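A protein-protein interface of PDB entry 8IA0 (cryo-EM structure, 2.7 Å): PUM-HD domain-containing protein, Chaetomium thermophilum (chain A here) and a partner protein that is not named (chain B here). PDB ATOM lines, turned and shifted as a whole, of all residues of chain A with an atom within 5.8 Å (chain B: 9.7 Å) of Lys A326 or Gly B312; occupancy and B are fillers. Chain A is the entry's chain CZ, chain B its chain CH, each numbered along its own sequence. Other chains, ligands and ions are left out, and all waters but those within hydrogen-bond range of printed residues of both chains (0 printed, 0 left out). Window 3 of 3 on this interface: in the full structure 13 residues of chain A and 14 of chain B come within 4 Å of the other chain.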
ATOM      1  N   ARG A 289      -7.097  23.618  -2.612  1.00  0.00           N
ATOM      2  CA  ARG A 289      -6.579  23.918  -3.943  1.00  0.00           C
ATOM      3  C   ARG A 289      -5.477  22.944  -4.339  1.00  0.00           C
ATOM      4  O   ARG A 289      -5.511  22.360  -5.428  1.00  0.00           O
ATOM      5  CB  ARG A 289      -6.065  25.357  -3.993  1.00  0.00           C
ATOM      6  CG  ARG A 289      -6.860  26.270  -4.908  1.00  0.00           C
ATOM      7  CD  ARG A 289      -6.058  27.491  -5.314  1.00  0.00           C
ATOM      8  NE  ARG A 289      -4.952  27.146  -6.198  1.00  0.00           N
ATOM      9  CZ  ARG A 289      -5.010  27.193  -7.522  1.00  0.00           C
ATOM     10  NH1 ARG A 289      -6.113  27.557  -8.153  1.00  0.00           N
ATOM     11  NH2 ARG A 289      -3.933  26.866  -8.230  1.00  0.00           N
ATOM     12  N   LEU A 323      -9.360  25.948 -16.262  1.00  0.00           N
ATOM     13  CA  LEU A 323      -9.979  27.203 -15.858  1.00  0.00           C
ATOM     14  C   LEU A 323      -9.457  27.669 -14.506  1.00  0.00           C
ATOM     15  O   LEU A 323      -9.264  28.870 -14.285  1.00  0.00           O
ATOM     16  CB  LEU A 323     -11.498  27.046 -15.823  1.00  0.00           C
ATOM     17  CG  LEU A 323     -12.324  28.246 -16.290  1.00  0.00           C
ATOM     18  CD1 LEU A 323     -11.713  28.870 -17.535  1.00  0.00           C
ATOM     19  CD2 LEU A 323     -13.765  27.832 -16.546  1.00  0.00           C
ATOM     20  N   ASN A 324      -9.226  26.734 -13.585  1.00  0.00           N
ATOM     21  CA  ASN A 324      -8.858  27.103 -12.226  1.00  0.00           C
ATOM     22  C   ASN A 324      -7.382  27.447 -12.071  1.00  0.00           C
ATOM     23  O   ASN A 324      -7.014  28.076 -11.073  1.00  0.00           O
ATOM     24  CB  ASN A 324      -9.232  25.977 -11.264  1.00  0.00           C
ATOM     25  CG  ASN A 324     -10.549  26.229 -10.569  1.00  0.00           C
ATOM     26  OD1 ASN A 324     -10.658  26.088  -9.350  1.00  0.00           O
ATOM     27  ND2 ASN A 324     -11.562  26.602 -11.339  1.00  0.00           N
ATOM     28  N   LEU A 325      -6.532  27.062 -13.021  1.00  0.00           N
ATOM     29  CA  LEU A 325      -5.124  27.437 -12.945  1.00  0.00           C
ATOM     30  C   LEU A 325      -4.962  28.946 -13.060  1.00  0.00           C
ATOM     31  O   LEU A 325      -5.666  29.611 -13.826  1.00  0.00           O
ATOM     32  CB  LEU A 325      -4.308  26.750 -14.043  1.00  0.00           C
ATOM     33  CG  LEU A 325      -3.691  25.362 -13.838  1.00  0.00           C
ATOM     34  CD1 LEU A 325      -4.577  24.450 -13.003  1.00  0.00           C
ATOM     35  CD2 LEU A 325      -3.357  24.725 -15.182  1.00  0.00           C
ATOM     36  N   LYS A 326      -4.031  29.483 -12.280  1.00  0.00           N
ATOM     37  CA  LYS A 326      -3.664  30.880 -12.411  1.00  0.00           C
ATOM     38  C   LYS A 326      -2.993  31.113 -13.764  1.00  0.00           C
ATOM     39  O   LYS A 326      -2.249  30.258 -14.251  1.00  0.00           O
ATOM     40  CB  LYS A 326      -2.733  31.288 -11.275  1.00  0.00           C
ATOM     41  CG  LYS A 326      -1.788  30.180 -10.835  1.00  0.00           C
ATOM     42  CD  LYS A 326      -1.151  30.490  -9.489  1.00  0.00           C
ATOM     43  CE  LYS A 326      -0.239  29.363  -9.025  1.00  0.00           C
ATOM     44  NZ  LYS A 326       0.946  29.195  -9.907  1.00  0.00           N
ATOM     45  N   PRO A 327      -3.254  32.257 -14.396  1.00  0.00           N
ATOM     46  CA  PRO A 327      -2.759  32.476 -15.760  1.00  0.00           C
ATOM     47  C   PRO A 327      -1.239  32.520 -15.828  1.00  0.00           C
ATOM     48  O   PRO A 327      -0.571  33.000 -14.911  1.00  0.00           O
ATOM     49  CB  PRO A 327      -3.377  33.825 -16.145  1.00  0.00           C
ATOM     50  CG  PRO A 327      -3.616  34.509 -14.844  1.00  0.00           C
ATOM     51  CD  PRO A 327      -4.004  33.418 -13.890  1.00  0.00           C
ATOM     52  N   GLU A 328      -0.702  32.001 -16.934  1.00  0.00           N
ATOM     53  CA  GLU A 328       0.721  32.063 -17.270  1.00  0.00           C
ATOM     54  C   GLU A 328       1.600  31.364 -16.233  1.00  0.00           C
ATOM     55  O   GLU A 328       2.823  31.531 -16.232  1.00  0.00           O
ATOM     56  CB  GLU A 328       1.170  33.519 -17.473  1.00  0.00           C
ATOM     57  CG  GLU A 328       2.342  33.702 -18.433  1.00  0.00           C
ATOM     58  CD  GLU A 328       3.658  33.949 -17.721  1.00  0.00           C
ATOM     59  OE1 GLU A 328       3.637  34.535 -16.619  1.00  0.00           O
ATOM     60  OE2 GLU A 328       4.712  33.555 -18.262  1.00  0.00           O
ATOM     61  N   SER A 329       1.003  30.575 -15.346  1.00  0.00           N
ATOM     62  CA  SER A 329       1.758  29.883 -14.316  1.00  0.00           C
ATOM     63  C   SER A 329       2.543  28.720 -14.918  1.00  0.00           C
ATOM     64  O   SER A 329       2.325  28.310 -16.060  1.00  0.00           O
ATOM     65  CB  SER A 329       0.828  29.379 -13.218  1.00  0.00           C
ATOM     66  OG  SER A 329      -0.008  28.342 -13.700  1.00  0.00           O
ATOM     67  N   GLU A 330       3.475  28.187 -14.125  1.00  0.00           N
ATOM     68  CA  GLU A 330       4.295  27.077 -14.595  1.00  0.00           C
ATOM     69  C   GLU A 330       3.426  25.857 -14.883  1.00  0.00           C
ATOM     70  O   GLU A 330       3.561  25.224 -15.936  1.00  0.00           O
ATOM     71  CB  GLU A 330       5.377  26.767 -13.553  1.00  0.00           C
ATOM     72  CG  GLU A 330       6.297  25.548 -13.774  1.00  0.00           C
ATOM     73  CD  GLU A 330       6.404  25.086 -15.218  1.00  0.00           C
ATOM     74  OE1 GLU A 330       7.053  25.785 -16.024  1.00  0.00           O
ATOM     75  OE2 GLU A 330       5.874  24.001 -15.537  1.00  0.00           O
ATOM     76  N   GLU A 331       2.482  25.550 -13.988  1.00  0.00           N
ATOM     77  CA  GLU A 331       1.611  24.400 -14.209  1.00  0.00           C
ATOM     78  C   GLU A 331       0.720  24.599 -15.429  1.00  0.00           C
ATOM     79  O   GLU A 331       0.305  23.619 -16.057  1.00  0.00           O
ATOM     80  CB  GLU A 331       0.761  24.127 -12.968  1.00  0.00           C
ATOM     81  CG  GLU A 331       1.433  24.500 -11.658  1.00  0.00           C
ATOM     82  CD  GLU A 331       0.986  25.853 -11.146  1.00  0.00           C
ATOM     83  OE1 GLU A 331       0.249  26.548 -11.876  1.00  0.00           O
ATOM     84  OE2 GLU A 331       1.375  26.224 -10.020  1.00  0.00           O
ATOM     85  N   LEU A 332       0.409  25.850 -15.775  1.00  0.00           N
ATOM     86  CA  LEU A 332      -0.295  26.109 -17.026  1.00  0.00           C
ATOM     87  C   LEU A 332       0.562  25.725 -18.224  1.00  0.00           C
ATOM     88  O   LEU A 332       0.059  25.147 -19.193  1.00  0.00           O
ATOM     89  CB  LEU A 332      -0.709  27.580 -17.102  1.00  0.00           C
ATOM     90  CG  LEU A 332      -1.628  28.004 -18.250  1.00  0.00           C
ATOM     91  CD1 LEU A 332      -2.623  29.044 -17.767  1.00  0.00           C
ATOM     92  CD2 LEU A 332      -0.827  28.553 -19.421  1.00  0.00           C
ATOM     93  N   PHE B 270      16.649  31.004  -1.878  1.00  0.00           N
ATOM     94  CA  PHE B 270      15.406  30.248  -1.990  1.00  0.00           C
ATOM     95  C   PHE B 270      15.378  29.410  -3.262  1.00  0.00           C
ATOM     96  O   PHE B 270      14.960  28.246  -3.237  1.00  0.00           O
ATOM     97  CB  PHE B 270      14.208  31.196  -1.950  1.00  0.00           C
ATOM     98  CG  PHE B 270      12.889  30.509  -2.148  1.00  0.00           C
ATOM     99  CD1 PHE B 270      12.288  29.824  -1.111  1.00  0.00           C
ATOM    100  CD2 PHE B 270      12.253  30.546  -3.376  1.00  0.00           C
ATOM    101  CE1 PHE B 270      11.078  29.192  -1.294  1.00  0.00           C
ATOM    102  CE2 PHE B 270      11.043  29.914  -3.564  1.00  0.00           C
ATOM    103  CZ  PHE B 270      10.455  29.236  -2.522  1.00  0.00           C
ATOM    104  N   LYS B 274      15.266  25.275  -3.508  1.00  0.00           N
ATOM    105  CA  LYS B 274      13.986  24.752  -3.980  1.00  0.00           C
ATOM    106  C   LYS B 274      14.039  23.281  -4.377  1.00  0.00           C
ATOM    107  O   LYS B 274      13.044  22.576  -4.132  1.00  0.00           O
ATOM    108  CB  LYS B 274      13.464  25.608  -5.140  1.00  0.00           C
ATOM    109  CG  LYS B 274      11.959  25.824  -5.099  1.00  0.00           C
ATOM    110  CD  LYS B 274      11.447  26.432  -6.391  1.00  0.00           C
ATOM    111  CE  LYS B 274      10.805  25.374  -7.275  1.00  0.00           C
ATOM    112  NZ  LYS B 274       9.765  24.597  -6.546  1.00  0.00           N
ATOM    113  N   PHE B 277      13.048  21.335  -1.582  1.00  0.00           N
ATOM    114  CA  PHE B 277      11.589  21.424  -1.505  1.00  0.00           C
ATOM    115  C   PHE B 277      10.946  20.804  -2.740  1.00  0.00           C
ATOM    116  O   PHE B 277      10.187  21.453  -3.456  1.00  0.00           O
ATOM    117  CB  PHE B 277      11.137  22.874  -1.348  1.00  0.00           C
ATOM    118  CG  PHE B 277      11.991  23.709  -0.432  1.00  0.00           C
ATOM    119  CD1 PHE B 277      12.629  23.162   0.668  1.00  0.00           C
ATOM    120  CD2 PHE B 277      12.079  25.075  -0.633  1.00  0.00           C
ATOM    121  CE1 PHE B 277      13.383  23.950   1.505  1.00  0.00           C
ATOM    122  CE2 PHE B 277      12.836  25.867   0.202  1.00  0.00           C
ATOM    123  CZ  PHE B 277      13.487  25.305   1.275  1.00  0.00           C
ATOM    124  N   ALA B 278      11.263  19.535  -3.004  1.00  0.00           N
ATOM    125  CA  ALA B 278      10.845  18.914  -4.257  1.00  0.00           C
ATOM    126  C   ALA B 278       9.328  18.800  -4.344  1.00  0.00           C
ATOM    127  O   ALA B 278       8.731  19.091  -5.387  1.00  0.00           O
ATOM    128  CB  ALA B 278      11.501  17.541  -4.404  1.00  0.00           C
ATOM    129  N   ASN B 279       8.684  18.383  -3.254  1.00  0.00           N
ATOM    130  CA  ASN B 279       7.240  18.187  -3.275  1.00  0.00           C
ATOM    131  C   ASN B 279       6.549  18.679  -2.010  1.00  0.00           C
ATOM    132  O   ASN B 279       5.351  18.424  -1.842  1.00  0.00           O
ATOM    133  CB  ASN B 279       6.908  16.706  -3.496  1.00  0.00           C
ATOM    134  CG  ASN B 279       7.890  15.781  -2.804  1.00  0.00           C
ATOM    135  OD1 ASN B 279       9.099  15.874  -3.011  1.00  0.00           O
ATOM    136  ND2 ASN B 279       7.372  14.882  -1.976  1.00  0.00           N
ATOM    137  N   LYS B 280       7.252  19.368  -1.119  1.00  0.00           N
ATOM    138  CA  LYS B 280       6.671  19.782   0.149  1.00  0.00           C
ATOM    139  C   LYS B 280       5.850  21.056  -0.043  1.00  0.00           C
ATOM    140  O   LYS B 280       5.812  21.650  -1.124  1.00  0.00           O
ATOM    141  CB  LYS B 280       7.764  19.962   1.197  1.00  0.00           C
ATOM    142  CG  LYS B 280       8.419  18.665   1.641  1.00  0.00           C
ATOM    143  CD  LYS B 280       9.659  18.933   2.476  1.00  0.00           C
ATOM    144  CE  LYS B 280      10.826  19.357   1.605  1.00  0.00           C
ATOM    145  NZ  LYS B 280      11.338  18.223   0.789  1.00  0.00           N
ATOM    146  N   MET B 281       5.182  21.486   1.021  1.00  0.00           N
ATOM    147  CA  MET B 281       4.388  22.710   1.030  1.00  0.00           C
ATOM    148  C   MET B 281       5.315  23.846   1.449  1.00  0.00           C
ATOM    149  O   MET B 281       5.790  23.884   2.585  1.00  0.00           O
ATOM    150  CB  MET B 281       3.205  22.568   1.979  1.00  0.00           C
ATOM    151  CG  MET B 281       2.369  21.322   1.737  1.00  0.00           C
ATOM    152  SD  MET B 281       0.832  21.280   2.677  1.00  0.00           S
ATOM    153  CE  MET B 281       0.960  22.792   3.623  1.00  0.00           C
ATOM    154  N   VAL B 282       5.571  24.771   0.531  1.00  0.00           N
ATOM    155  CA  VAL B 282       6.520  25.854   0.756  1.00  0.00           C
ATOM    156  C   VAL B 282       5.744  27.145   0.966  1.00  0.00           C
ATOM    157  O   VAL B 282       4.899  27.514   0.142  1.00  0.00           O
ATOM    158  CB  VAL B 282       7.507  25.988  -0.412  1.00  0.00           C
ATOM    159  CG1 VAL B 282       8.607  26.967  -0.057  1.00  0.00           C
ATOM    160  CG2 VAL B 282       8.084  24.634  -0.764  1.00  0.00           C
ATOM    161  N   ASN B 306       6.732  38.574  -6.004  1.00  0.00           N
ATOM    162  CA  ASN B 306       5.450  38.041  -6.453  1.00  0.00           C
ATOM    163  C   ASN B 306       5.632  36.877  -7.419  1.00  0.00           C
ATOM    164  O   ASN B 306       4.915  35.874  -7.328  1.00  0.00           O
ATOM    165  CB  ASN B 306       4.617  39.146  -7.101  1.00  0.00           C
ATOM    166  CG  ASN B 306       3.876  39.989  -6.084  1.00  0.00           C
ATOM    167  OD1 ASN B 306       3.774  39.622  -4.915  1.00  0.00           O
ATOM    168  ND2 ASN B 306       3.351  41.126  -6.527  1.00  0.00           N
ATOM    169  N   ASP B 307       6.580  36.985  -8.353  1.00  0.00           N
ATOM    170  CA  ASP B 307       6.736  35.918  -9.337  1.00  0.00           C
ATOM    171  C   ASP B 307       7.319  34.653  -8.720  1.00  0.00           C
ATOM    172  O   ASP B 307       7.319  33.598  -9.365  1.00  0.00           O
ATOM    173  CB  ASP B 307       7.570  36.403 -10.533  1.00  0.00           C
ATOM    174  CG  ASP B 307       9.059  36.546 -10.228  1.00  0.00           C
ATOM    175  OD1 ASP B 307       9.510  36.235  -9.109  1.00  0.00           O
ATOM    176  OD2 ASP B 307       9.794  36.981 -11.138  1.00  0.00           O
ATOM    177  N   LEU B 308       7.828  34.740  -7.489  1.00  0.00           N
ATOM    178  CA  LEU B 308       8.189  33.537  -6.749  1.00  0.00           C
ATOM    179  C   LEU B 308       6.950  32.706  -6.445  1.00  0.00           C
ATOM    180  O   LEU B 308       6.959  31.478  -6.577  1.00  0.00           O
ATOM    181  CB  LEU B 308       8.920  33.917  -5.461  1.00  0.00           C
ATOM    182  CG  LEU B 308      10.446  33.955  -5.535  1.00  0.00           C
ATOM    183  CD1 LEU B 308      11.034  34.306  -4.179  1.00  0.00           C
ATOM    184  CD2 LEU B 308      10.994  32.631  -6.036  1.00  0.00           C
ATOM    185  N   THR B 309       5.871  33.371  -6.026  1.00  0.00           N
ATOM    186  CA  THR B 309       4.581  32.699  -5.905  1.00  0.00           C
ATOM    187  C   THR B 309       4.094  32.228  -7.267  1.00  0.00           C
ATOM    188  O   THR B 309       3.459  31.173  -7.383  1.00  0.00           O
ATOM    189  CB  THR B 309       3.564  33.642  -5.256  1.00  0.00           C
ATOM    190  OG1 THR B 309       3.732  33.620  -3.833  1.00  0.00           O
ATOM    191  CG2 THR B 309       2.135  33.238  -5.594  1.00  0.00           C
ATOM    192  N   LYS B 310       4.428  32.976  -8.315  1.00  0.00           N
ATOM    193  CA  LYS B 310       4.032  32.652  -9.678  1.00  0.00           C
ATOM    194  C   LYS B 310       4.999  31.595 -10.213  1.00  0.00           C
ATOM    195  O   LYS B 310       5.581  31.731 -11.295  1.00  0.00           O
ATOM    196  CB  LYS B 310       4.013  33.957 -10.491  1.00  0.00           C
ATOM    197  CG  LYS B 310       3.830  33.889 -11.992  1.00  0.00           C
ATOM    198  CD  LYS B 310       2.463  33.402 -12.387  1.00  0.00           C
ATOM    199  CE  LYS B 310       2.251  33.699 -13.849  1.00  0.00           C
ATOM    200  NZ  LYS B 310       3.396  33.190 -14.651  1.00  0.00           N
ATOM    201  N   SER B 311       5.187  30.538  -9.424  1.00  0.00           N
ATOM    202  CA  SER B 311       6.033  29.404  -9.786  1.00  0.00           C
ATOM    203  C   SER B 311       5.769  28.315  -8.755  1.00  0.00           C
ATOM    204  O   SER B 311       6.047  28.513  -7.568  1.00  0.00           O
ATOM    205  CB  SER B 311       7.511  29.789  -9.813  1.00  0.00           C
ATOM    206  OG  SER B 311       7.891  30.435  -8.611  1.00  0.00           O
ATOM    207  N   GLY B 312       5.239  27.180  -9.192  1.00  0.00           N
ATOM    208  CA  GLY B 312       4.926  26.125  -8.251  1.00  0.00           C
ATOM    209  C   GLY B 312       3.717  26.469  -7.397  1.00  0.00           C
ATOM    210  O   GLY B 312       2.798  27.179  -7.816  1.00  0.00           O
ATOM    211  N   GLU B 313       3.734  25.962  -6.166  1.00  0.00           N
ATOM    212  CA  GLU B 313       2.626  26.120  -5.231  1.00  0.00           C
ATOM    213  C   GLU B 313       3.052  26.850  -3.960  1.00  0.00           C
ATOM    214  O   GLU B 313       2.738  26.427  -2.846  1.00  0.00           O
ATOM    215  CB  GLU B 313       2.018  24.763  -4.884  1.00  0.00           C
ATOM    216  CG  GLU B 313       0.951  24.270  -5.860  1.00  0.00           C
ATOM    217  CD  GLU B 313      -0.048  25.343  -6.271  1.00  0.00           C
ATOM    218  OE1 GLU B 313      -0.417  26.190  -5.428  1.00  0.00           O
ATOM    219  OE2 GLU B 313      -0.466  25.338  -7.448  1.00  0.00           O
ATOM    220  N   VAL B 314       3.773  27.957  -4.112  1.00  0.00           N
ATOM    221  CA  VAL B 314       4.293  28.696  -2.969  1.00  0.00           C
ATOM    222  C   VAL B 314       3.355  29.846  -2.635  1.00  0.00           C
ATOM    223  O   VAL B 314       2.971  30.632  -3.509  1.00  0.00           O
ATOM    224  CB  VAL B 314       5.715  29.205  -3.266  1.00  0.00           C
ATOM    225  CG1 VAL B 314       6.168  30.183  -2.194  1.00  0.00           C
ATOM    226  CG2 VAL B 314       6.679  28.038  -3.388  1.00  0.00           C
ATOM    227  N   GLU B 315       2.981  29.949  -1.362  1.00  0.00           N
ATOM    228  CA  GLU B 315       2.128  31.022  -0.865  1.00  0.00           C
ATOM    229  C   GLU B 315       2.978  32.003  -0.073  1.00  0.00           C
ATOM    230  O   GLU B 315       3.944  31.602   0.585  1.00  0.00           O
ATOM    231  CB  GLU B 315       0.993  30.487   0.019  1.00  0.00           C
ATOM    232  CG  GLU B 315       0.289  29.173  -0.396  1.00  0.00           C
ATOM    233  CD  GLU B 315       0.246  28.870  -1.895  1.00  0.00           C
ATOM    234  OE1 GLU B 315       0.208  29.803  -2.726  1.00  0.00           O
ATOM    235  OE2 GLU B 315       0.239  27.671  -2.241  1.00  0.00           O
ATOM    236  N   ARG B 337      -3.497  23.871   6.138  1.00  0.00           N
ATOM    237  CA  ARG B 337      -3.129  23.295   4.852  1.00  0.00           C
ATOM    238  C   ARG B 337      -2.423  21.958   5.028  1.00  0.00           C
ATOM    239  O   ARG B 337      -2.584  21.052   4.203  1.00  0.00           O
ATOM    240  CB  ARG B 337      -2.263  24.286   4.079  1.00  0.00           C
ATOM    241  CG  ARG B 337      -3.051  25.143   3.105  1.00  0.00           C
ATOM    242  CD  ARG B 337      -2.275  25.399   1.834  1.00  0.00           C
ATOM    243  NE  ARG B 337      -1.520  24.226   1.413  1.00  0.00           N
ATOM    244  CZ  ARG B 337      -0.746  24.182   0.338  1.00  0.00           C
ATOM    245  NH1 ARG B 337      -0.614  25.229  -0.460  1.00  0.00           N
ATOM    246  NH2 ARG B 337      -0.087  23.063   0.057  1.00  0.00           N
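Printed residues of chain B within 4 Å of Arg A289: Glu B313 (3.9 Å). Lys A326 touches just one residue of chain B: Gly B312. Pro A327 touches just one residue of chain B: Lys B310 (3.1 Å). Printed residues of chain B within 4 Å of Glu A328: Lys B310 (2.4 Å). Of the printed residues of chain B, Ser A329 touches Lys B310. Printed residues of chain B within 4 Å of Glu A331: Gly B312 (2.8 Å) and Glu B313 (3.3 Å). Of the printed residues of chain A, Lys B310 touches Pro A327, Glu A328 and Ser A329. Of chain A, only Lys A326 and Glu A331 come within 4 Å of Gly B312. Of the printed residues of chain A, Glu B313 touches Arg A289 (3.9 Å) and Glu A331 (3.3 Å). The nearest residue of chain B that does not touch Lys A326 is Thr B309 (4.1 Å).
Among the printed residues, merely in contact across the chains: Pro A327 with Lys B310 (3.1 Å) and Ser A329 with Lys B310 (3.6 Å).
Of the 19 printed residues of chain B, 3 touch a printed residue of chain A. Among the printed residues, 7 pairs touch across the chains. Among the printed residues, Asp or Glu carboxylates within 4 Å of a Lys or Arg side-chain nitrogen of the other chain: Arg A289 with Glu B313 and Glu A328 with Lys B310.
OG of Ser A329 is in hydrogen-bond range of OE1 of Glu A331, at 2.6 Å. The side-chain hydroxyl (OG) of Ser A329 is in hydrogen-bond range of the backbone NH (N) of Leu A332, at 3.3 Å. The backbone carbonyl oxygen of Lys A326 sits at hydrogen-bond distance from the side-chain hydroxyl of Ser A329. NZ of Lys A326 is in salt-bridge range of OE2 of Glu A331. The backbone carbonyl oxygen (O) of Asn A324 is in hydrogen-bond range of the guanidinium group (NH1) of Arg A289.
The backbone carbonyl oxygen of Gly B312 lies close to the side-chain carboxylate of Glu A331 (2.8 Å). OE2 of Glu A328 is in salt-bridge range of NZ of Lys B310, at 3.9 Å. The backbone carbonyl oxygen (O) of Gly B312 lies within hydrogen-bond range of the side-chain amino group (NZ) of Lys A326, at 3.4 Å. The side-chain carboxylate (OE2) of Glu A331 lies close to the side-chain carboxylate (OE2) of Glu B313 (3.3 Å). The guanidinium group (NH2) of Arg A289 lies within salt-bridge range of the side-chain carboxylate (OE2) of Glu B313 (3.9 Å).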
